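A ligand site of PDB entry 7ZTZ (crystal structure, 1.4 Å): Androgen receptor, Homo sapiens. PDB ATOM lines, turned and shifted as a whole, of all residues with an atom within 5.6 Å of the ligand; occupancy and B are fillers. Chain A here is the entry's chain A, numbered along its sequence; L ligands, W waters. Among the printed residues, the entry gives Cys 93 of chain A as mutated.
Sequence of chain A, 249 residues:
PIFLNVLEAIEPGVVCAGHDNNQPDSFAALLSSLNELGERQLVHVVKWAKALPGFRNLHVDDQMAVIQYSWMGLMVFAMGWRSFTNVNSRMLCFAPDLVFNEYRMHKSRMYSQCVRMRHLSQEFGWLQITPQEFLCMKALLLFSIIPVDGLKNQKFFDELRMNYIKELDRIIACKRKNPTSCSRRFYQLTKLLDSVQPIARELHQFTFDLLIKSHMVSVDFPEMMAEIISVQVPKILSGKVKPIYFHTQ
The side-chain amide oxygen of Asn 35 is in hydrogen-bond range of an oxygen (O2) of the ligand.
The side-chain hydroxyl (OG1) of Thr 207 sits at hydrogen-bond distance from an oxygen (O2) of the ligand, at 2.7 Å.
O1 of the ligand lies within hydrogen-bond range of NH2 of Arg 82 (3.1 Å).
NE2 of Gln 41 sits at hydrogen-bond distance from O1 of the ligand.
O of Leu 31 sits close to ND2 of Asn 35, 3.4 Å away.
The guanidinium group (NH2) of Arg 82 sits close to the side-chain amide nitrogen (NE2) of Gln 41 (3.3 Å).
The guanidinium group of Arg 82 is in hydrogen-bond range of the backbone carbonyl oxygen of Phe 94 (2.8 Å).
O of Cys 93 is in hydrogen-bond range of NE of Arg 82 (3.2 Å).
The side-chain amide oxygen (OE1) of Gln 41 sits close to the side-chain sulfur (SD) of Met 75, at 3.7 Å.
Leu 31 touches the ligand.
Leu 34 touches the ligand (O to C11, 3.4 Å).
Leu 37 touches the ligand (CD2 to C2, 3.9 Å).
CE of Met 72 touches C18 of the ligand (3.8 Å).
Met 75 touches the ligand (SD to C19, 3.7 Å).
Met 79 touches the ligand (CB to O1, 3.6 Å).
Phe 94 touches the ligand.
SD of Met 110 touches C15 of the ligand, 3.8 Å away.
CD1 of Phe 206 touches C16 of the ligand, 3.9 Å away.
Phe 221 touches the ligand.
CE of Met 225 touches C12 of the ligand (3.7 Å).
Hydrophobic or aromatic side chains within 4 Å of the ligand: Leu 31, Leu 34, Leu 37, Met 72, Met 75, Met 79, Phe 94, Met 110, Phe 206, Phe 221 and Met 225.
Along chain A the residues within 4 Å of the ligand span positions 31 to 225.
The nearest printed residue that does not touch the ligand is Val 76 (4.1 Å).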
ATOM      1  N   LEU A  31      28.681 -37.355  21.919  1.00  0.00           N
ATOM      2  CA  LEU A  31      28.541 -35.908  21.866  1.00  0.00           C
ATOM      3  C   LEU A  31      27.067 -35.514  21.746  1.00  0.00           C
ATOM      4  O   LEU A  31      26.636 -34.498  22.320  1.00  0.00           O
ATOM      5  CB  LEU A  31      29.389 -35.294  20.731  1.00  0.00           C
ATOM      6  CG  LEU A  31      30.808 -34.918  21.127  1.00  0.00           C
ATOM      7  CD1 LEU A  31      30.838 -33.704  22.046  1.00  0.00           C
ATOM      8  CD2 LEU A  31      31.522 -36.088  21.818  1.00  0.00           C
ATOM      9  N   LEU A  34      26.013 -35.604  25.305  1.00  0.00           N
ATOM     10  CA  LEU A  34      26.485 -34.436  26.038  1.00  0.00           C
ATOM     11  C   LEU A  34      25.698 -33.181  25.671  1.00  0.00           C
ATOM     12  O   LEU A  34      25.416 -32.347  26.538  1.00  0.00           O
ATOM     13  CB  LEU A  34      27.981 -34.208  25.758  1.00  0.00           C
ATOM     14  CG  LEU A  34      28.905 -35.141  26.534  1.00  0.00           C
ATOM     15  CD1 LEU A  34      30.339 -34.978  25.993  1.00  0.00           C
ATOM     16  CD2 LEU A  34      28.891 -34.822  28.014  1.00  0.00           C
ATOM     17  N   ASN A  35      25.323 -33.047  24.374  1.00  0.00           N
ATOM     18  CA  ASN A  35      24.576 -31.865  23.994  1.00  0.00           C
ATOM     19  C   ASN A  35      23.188 -31.840  24.627  1.00  0.00           C
ATOM     20  O   ASN A  35      22.719 -30.788  25.045  1.00  0.00           O
ATOM     21  CB  ASN A  35      24.474 -31.768  22.477  1.00  0.00           C
ATOM     22  CG  ASN A  35      25.766 -31.412  21.787  1.00  0.00           C
ATOM     23  OD1 ASN A  35      26.618 -30.792  22.411  1.00  0.00           O
ATOM     24  ND2 ASN A  35      25.848 -31.728  20.502  1.00  0.00           N
ATOM     25  N   LEU A  37      22.452 -33.310  27.454  1.00  0.00           N
ATOM     26  CA  LEU A  37      22.668 -32.982  28.851  1.00  0.00           C
ATOM     27  C   LEU A  37      22.812 -31.472  29.033  1.00  0.00           C
ATOM     28  O   LEU A  37      22.327 -30.888  29.993  1.00  0.00           O
ATOM     29  CB  LEU A  37      23.932 -33.683  29.379  1.00  0.00           C
ATOM     30  CG  LEU A  37      24.311 -33.441  30.838  1.00  0.00           C
ATOM     31  CD1 LEU A  37      23.183 -33.950  31.789  1.00  0.00           C
ATOM     32  CD2 LEU A  37      25.562 -34.226  31.156  1.00  0.00           C
ATOM     33  N   GLY A  38      23.570 -30.851  28.106  1.00  0.00           N
ATOM     34  CA  GLY A  38      23.703 -29.406  28.167  1.00  0.00           C
ATOM     35  C   GLY A  38      22.368 -28.670  28.100  1.00  0.00           C
ATOM     36  O   GLY A  38      22.128 -27.768  28.901  1.00  0.00           O
ATOM     37  N   GLN A  41      20.569 -29.278  31.439  1.00  0.00           N
ATOM     38  CA  GLN A  41      21.181 -28.548  32.534  1.00  0.00           C
ATOM     39  C   GLN A  41      20.878 -27.055  32.408  1.00  0.00           C
ATOM     40  O   GLN A  41      20.760 -26.378  33.413  1.00  0.00           O
ATOM     41  CB  GLN A  41      22.715 -28.802  32.597  1.00  0.00           C
ATOM     42  CG  GLN A  41      23.049 -30.168  33.230  1.00  0.00           C
ATOM     43  CD  GLN A  41      24.471 -30.349  33.662  1.00  0.00           C
ATOM     44  OE1 GLN A  41      25.213 -29.379  33.789  1.00  0.00           O
ATOM     45  NE2 GLN A  41      24.841 -31.587  33.944  1.00  0.00           N
ATOM     46  N   TRP A  71      27.471 -20.195  31.221  1.00  0.00           N
ATOM     47  CA  TRP A  71      26.958 -21.546  31.440  1.00  0.00           C
ATOM     48  C   TRP A  71      28.032 -22.627  31.334  1.00  0.00           C
ATOM     49  O   TRP A  71      27.982 -23.598  32.072  1.00  0.00           O
ATOM     50  CB  TRP A  71      25.794 -21.919  30.523  1.00  0.00           C
ATOM     51  CG  TRP A  71      26.190 -21.896  29.077  1.00  0.00           C
ATOM     52  CD1 TRP A  71      26.155 -20.786  28.278  1.00  0.00           C
ATOM     53  CD2 TRP A  71      26.633 -22.986  28.249  1.00  0.00           C
ATOM     54  NE1 TRP A  71      26.594 -21.111  27.027  1.00  0.00           N
ATOM     55  CE2 TRP A  71      26.874 -22.458  26.960  1.00  0.00           C
ATOM     56  CE3 TRP A  71      26.870 -24.359  28.461  1.00  0.00           C
ATOM     57  CZ2 TRP A  71      27.343 -23.233  25.891  1.00  0.00           C
ATOM     58  CZ3 TRP A  71      27.237 -25.129  27.387  1.00  0.00           C
ATOM     59  CH2 TRP A  71      27.529 -24.587  26.131  1.00  0.00           C
ATOM     60  N   MET A  72      28.979 -22.487  30.408  1.00  0.00           N
ATOM     61  CA  MET A  72      29.940 -23.572  30.204  1.00  0.00           C
ATOM     62  C   MET A  72      30.781 -23.710  31.483  1.00  0.00           C
ATOM     63  O   MET A  72      30.915 -24.818  32.016  1.00  0.00           O
ATOM     64  CB  MET A  72      30.845 -23.244  28.984  1.00  0.00           C
ATOM     65  CG  MET A  72      31.896 -24.403  28.755  1.00  0.00           C
ATOM     66  SD  MET A  72      31.161 -25.847  28.015  1.00  0.00           S
ATOM     67  CE  MET A  72      31.054 -25.227  26.330  1.00  0.00           C
ATOM     68  N   MET A  75      28.761 -25.188  34.428  1.00  0.00           N
ATOM     69  CA  MET A  75      28.405 -26.575  34.287  1.00  0.00           C
ATOM     70  C   MET A  75      29.685 -27.410  34.481  1.00  0.00           C
ATOM     71  O   MET A  75      29.594 -28.488  35.058  1.00  0.00           O
ATOM     72  CB  MET A  75      27.801 -26.890  32.937  1.00  0.00           C
ATOM     73  CG  MET A  75      26.349 -26.338  32.813  1.00  0.00           C
ATOM     74  SD  MET A  75      25.686 -26.778  31.202  1.00  0.00           S
ATOM     75  CE  MET A  75      24.151 -25.828  31.279  1.00  0.00           C
ATOM     76  N   VAL A  76      30.828 -26.944  34.003  1.00  0.00           N
ATOM     77  CA  VAL A  76      32.074 -27.710  34.174  1.00  0.00           C
ATOM     78  C   VAL A  76      32.462 -27.734  35.648  1.00  0.00           C
ATOM     79  O   VAL A  76      32.882 -28.780  36.215  1.00  0.00           O
ATOM     80  CB  VAL A  76      33.184 -27.056  33.343  1.00  0.00           C
ATOM     81  CG1 VAL A  76      34.567 -27.552  33.787  1.00  0.00           C
ATOM     82  CG2 VAL A  76      33.013 -27.344  31.861  1.00  0.00           C
ATOM     83  N   MET A  79      30.182 -30.133  37.438  1.00  0.00           N
ATOM     84  CA  MET A  79      30.499 -31.502  37.071  1.00  0.00           C
ATOM     85  C   MET A  79      31.751 -31.929  37.814  1.00  0.00           C
ATOM     86  O   MET A  79      31.811 -33.076  38.327  1.00  0.00           O
ATOM     87  CB  MET A  79      30.658 -31.630  35.553  1.00  0.00           C
ATOM     88  CG  MET A  79      30.884 -33.011  35.092  1.00  0.00           C
ATOM     89  SD  MET A  79      32.634 -33.484  35.144  1.00  0.00           S
ATOM     90  CE  MET A  79      33.249 -32.412  33.829  1.00  0.00           C
ATOM     91  N   ARG A  82      30.666 -32.827  41.336  1.00  0.00           N
ATOM     92  CA  ARG A  82      29.948 -34.099  41.346  1.00  0.00           C
ATOM     93  C   ARG A  82      30.942 -35.244  41.167  1.00  0.00           C
ATOM     94  O   ARG A  82      30.801 -36.299  41.815  1.00  0.00           O
ATOM     95  CB  ARG A  82      29.024 -34.217  40.127  1.00  0.00           C
ATOM     96  CG  ARG A  82      27.794 -33.357  40.239  1.00  0.00           C
ATOM     97  CD  ARG A  82      26.856 -33.964  39.209  1.00  0.00           C
ATOM     98  NE  ARG A  82      27.113 -33.784  37.794  1.00  0.00           N
ATOM     99  CZ  ARG A  82      27.040 -32.601  37.158  1.00  0.00           C
ATOM    100  NH1 ARG A  82      26.803 -31.465  37.825  1.00  0.00           N
ATOM    101  NH2 ARG A  82      27.302 -32.572  35.881  1.00  0.00           N
ATOM    102  N   CYS A  93      31.913 -37.491  35.898  1.00  0.00           N
ATOM    103  CA  CYS A  93      30.516 -37.811  36.144  1.00  0.00           C
ATOM    104  C   CYS A  93      29.641 -36.705  35.579  1.00  0.00           C
ATOM    105  O   CYS A  93      29.096 -35.886  36.323  1.00  0.00           O
ATOM    106  CB  CYS A  93      30.259 -37.920  37.632  1.00  0.00           C
ATOM    107  SG  CYS A  93      31.165 -39.297  38.417  1.00  0.00           S
ATOM    108  N   PHE A  94      29.476 -36.751  34.277  1.00  0.00           N
ATOM    109  CA  PHE A  94      28.664 -35.713  33.612  1.00  0.00           C
ATOM    110  C   PHE A  94      27.214 -35.841  34.095  1.00  0.00           C
ATOM    111  O   PHE A  94      26.545 -34.870  34.425  1.00  0.00           O
ATOM    112  CB  PHE A  94      28.726 -35.899  32.103  1.00  0.00           C
ATOM    113  CG  PHE A  94      30.058 -35.539  31.502  1.00  0.00           C
ATOM    114  CD1 PHE A  94      30.453 -34.214  31.404  1.00  0.00           C
ATOM    115  CD2 PHE A  94      30.920 -36.519  31.026  1.00  0.00           C
ATOM    116  CE1 PHE A  94      31.680 -33.848  30.863  1.00  0.00           C
ATOM    117  CE2 PHE A  94      32.131 -36.160  30.443  1.00  0.00           C
ATOM    118  CZ  PHE A  94      32.551 -34.830  30.407  1.00  0.00           C
ATOM    119  N   MET A 110      37.762 -35.652  22.982  1.00  0.00           N
ATOM    120  CA  MET A 110      37.994 -34.622  23.983  1.00  0.00           C
ATOM    121  C   MET A 110      38.960 -35.061  25.070  1.00  0.00           C
ATOM    122  O   MET A 110      38.920 -34.584  26.207  1.00  0.00           O
ATOM    123  CB  MET A 110      36.654 -34.242  24.622  1.00  0.00           C
ATOM    124  CG  MET A 110      35.930 -33.371  23.649  1.00  0.00           C
ATOM    125  SD  MET A 110      34.562 -32.516  24.437  1.00  0.00           S
ATOM    126  CE  MET A 110      33.686 -33.969  24.895  1.00  0.00           C
ATOM    127  N   MET A 117      39.655 -31.265  32.839  1.00  0.00           N
ATOM    128  CA  MET A 117      38.502 -31.309  33.723  1.00  0.00           C
ATOM    129  C   MET A 117      38.695 -32.227  34.927  1.00  0.00           C
ATOM    130  O   MET A 117      38.273 -31.963  36.054  1.00  0.00           O
ATOM    131  CB  MET A 117      37.240 -31.680  32.964  1.00  0.00           C
ATOM    132  CG  MET A 117      36.793 -30.517  32.042  1.00  0.00           C
ATOM    133  SD  MET A 117      35.161 -30.866  31.295  1.00  0.00           S
ATOM    134  CE  MET A 117      35.610 -31.930  29.927  1.00  0.00           C
ATOM    135  N   LEU A 203      36.497 -25.613  25.687  1.00  0.00           N
ATOM    136  CA  LEU A 203      35.257 -26.305  25.343  1.00  0.00           C
ATOM    137  C   LEU A 203      34.384 -25.418  24.449  1.00  0.00           C
ATOM    138  O   LEU A 203      33.698 -25.933  23.552  1.00  0.00           O
ATOM    139  CB  LEU A 203      34.486 -26.690  26.609  1.00  0.00           C
ATOM    140  CG  LEU A 203      35.229 -27.722  27.445  1.00  0.00           C
ATOM    141  CD1 LEU A 203      34.642 -27.877  28.811  1.00  0.00           C
ATOM    142  CD2 LEU A 203      35.267 -29.064  26.711  1.00  0.00           C
ATOM    143  N   PHE A 206      35.780 -26.056  21.075  1.00  0.00           N
ATOM    144  CA  PHE A 206      35.441 -27.377  20.562  1.00  0.00           C
ATOM    145  C   PHE A 206      33.990 -27.462  20.098  1.00  0.00           C
ATOM    146  O   PHE A 206      33.645 -28.046  19.072  1.00  0.00           O
ATOM    147  CB  PHE A 206      35.745 -28.388  21.687  1.00  0.00           C
ATOM    148  CG  PHE A 206      35.606 -29.836  21.283  1.00  0.00           C
ATOM    149  CD1 PHE A 206      34.388 -30.478  21.337  1.00  0.00           C
ATOM    150  CD2 PHE A 206      36.713 -30.529  20.788  1.00  0.00           C
ATOM    151  CE1 PHE A 206      34.244 -31.787  20.887  1.00  0.00           C
ATOM    152  CE2 PHE A 206      36.592 -31.839  20.372  1.00  0.00           C
ATOM    153  CZ  PHE A 206      35.361 -32.476  20.442  1.00  0.00           C
ATOM    154  N   THR A 207      33.091 -26.946  20.926  1.00  0.00           N
ATOM    155  CA  THR A 207      31.675 -27.056  20.606  1.00  0.00           C
ATOM    156  C   THR A 207      31.262 -26.194  19.399  1.00  0.00           C
ATOM    157  O   THR A 207      30.437 -26.614  18.613  1.00  0.00           O
ATOM    158  CB  THR A 207      30.824 -26.757  21.860  1.00  0.00           C
ATOM    159  OG1 THR A 207      29.498 -27.283  21.623  1.00  0.00           O
ATOM    160  CG2 THR A 207      30.656 -25.282  22.235  1.00  0.00           C
ATOM    161  N   LEU A 210      32.407 -28.046  16.442  1.00  0.00           N
ATOM    162  CA  LEU A 210      31.576 -29.227  16.258  1.00  0.00           C
ATOM    163  C   LEU A 210      30.214 -28.820  15.672  1.00  0.00           C
ATOM    164  O   LEU A 210      29.720 -29.523  14.807  1.00  0.00           O
ATOM    165  CB  LEU A 210      31.420 -29.952  17.594  1.00  0.00           C
ATOM    166  CG  LEU A 210      30.515 -31.183  17.604  1.00  0.00           C
ATOM    167  CD1 LEU A 210      31.009 -32.218  16.593  1.00  0.00           C
ATOM    168  CD2 LEU A 210      30.510 -31.800  18.991  1.00  0.00           C
ATOM    169  N   PHE A 221      22.518 -31.282  17.773  1.00  0.00           N
ATOM    170  CA  PHE A 221      22.459 -30.201  18.739  1.00  0.00           C
ATOM    171  C   PHE A 221      21.002 -29.791  18.963  1.00  0.00           C
ATOM    172  O   PHE A 221      20.343 -29.384  18.011  1.00  0.00           O
ATOM    173  CB  PHE A 221      23.193 -28.941  18.254  1.00  0.00           C
ATOM    174  CG  PHE A 221      24.687 -29.052  18.417  1.00  0.00           C
ATOM    175  CD1 PHE A 221      25.477 -29.758  17.510  1.00  0.00           C
ATOM    176  CD2 PHE A 221      25.317 -28.404  19.464  1.00  0.00           C
ATOM    177  CE1 PHE A 221      26.859 -29.845  17.663  1.00  0.00           C
ATOM    178  CE2 PHE A 221      26.700 -28.465  19.585  1.00  0.00           C
ATOM    179  CZ  PHE A 221      27.467 -29.191  18.720  1.00  0.00           C
ATOM    180  N   MET A 225      20.903 -25.083  22.716  1.00  0.00           N
ATOM    181  CA  MET A 225      22.356 -25.252  22.517  1.00  0.00           C
ATOM    182  C   MET A 225      22.767 -24.688  21.168  1.00  0.00           C
ATOM    183  O   MET A 225      23.751 -23.946  21.089  1.00  0.00           O
ATOM    184  CB  MET A 225      22.806 -26.715  22.671  1.00  0.00           C
ATOM    185  CG  MET A 225      22.600 -27.229  24.117  1.00  0.00           C
ATOM    186  SD  MET A 225      23.898 -26.646  25.222  1.00  0.00           S
ATOM    187  CE  MET A 225      25.198 -27.785  24.768  1.00  0.00           C
ATOM    188  N   ILE A 229      25.283 -21.521  21.010  1.00  0.00           N
ATOM    189  CA  ILE A 229      26.601 -21.783  20.452  1.00  0.00           C
ATOM    190  C   ILE A 229      26.849 -20.990  19.175  1.00  0.00           C
ATOM    191  O   ILE A 229      28.036 -20.711  18.912  1.00  0.00           O
ATOM    192  CB  ILE A 229      26.870 -23.289  20.344  1.00  0.00           C
ATOM    193  CG1 ILE A 229      26.873 -23.851  21.780  1.00  0.00           C
ATOM    194  CG2 ILE A 229      28.217 -23.510  19.674  1.00  0.00           C
ATOM    195  CD1 ILE A 229      26.672 -25.371  21.816  1.00  0.00           C
HETATM  196  C1  LIG L   1      27.306 -30.764  29.769  1.00  0.00           C
HETATM  197  C2  LIG L   1      27.042 -30.618  31.254  1.00  0.00           C
HETATM  198  C3  LIG L   1      28.226 -31.043  32.060  1.00  0.00           C
HETATM  199  O1  LIG L   1      28.118 -31.751  33.037  1.00  0.00           O
HETATM  200  C4  LIG L   1      29.548 -30.523  31.617  1.00  0.00           C
HETATM  201  C5  LIG L   1      29.747 -30.675  30.100  1.00  0.00           C
HETATM  202  C6  LIG L   1      31.121 -30.181  29.614  1.00  0.00           C
HETATM  203  C7  LIG L   1      31.283 -30.528  28.133  1.00  0.00           C
HETATM  204  C8  LIG L   1      30.194 -29.924  27.256  1.00  0.00           C
HETATM  205  C9  LIG L   1      28.795 -30.385  27.770  1.00  0.00           C
HETATM  206  C10 LIG L   1      28.599 -30.047  29.275  1.00  0.00           C
HETATM  207  C11 LIG L   1      27.669 -29.833  26.861  1.00  0.00           C
HETATM  208  C12 LIG L   1      27.895 -30.254  25.401  1.00  0.00           C
HETATM  209  C13 LIG L   1      29.264 -29.778  24.891  1.00  0.00           C
HETATM  210  C14 LIG L   1      30.332 -30.371  25.806  1.00  0.00           C
HETATM  211  C15 LIG L   1      31.676 -30.132  25.061  1.00  0.00           C
HETATM  212  C16 LIG L   1      31.255 -30.297  23.587  1.00  0.00           C
HETATM  213  C17 LIG L   1      29.723 -30.419  23.583  1.00  0.00           C
HETATM  214  O2  LIG L   1      29.178 -29.877  22.389  1.00  0.00           O
HETATM  215  C18 LIG L   1      29.291 -28.235  24.779  1.00  0.00           C
HETATM  216  C19 LIG L   1      28.467 -28.518  29.454  1.00  0.00           C
HETATM  217  O   HOH W   1      27.112 -29.624  35.504  1.00  0.00           O
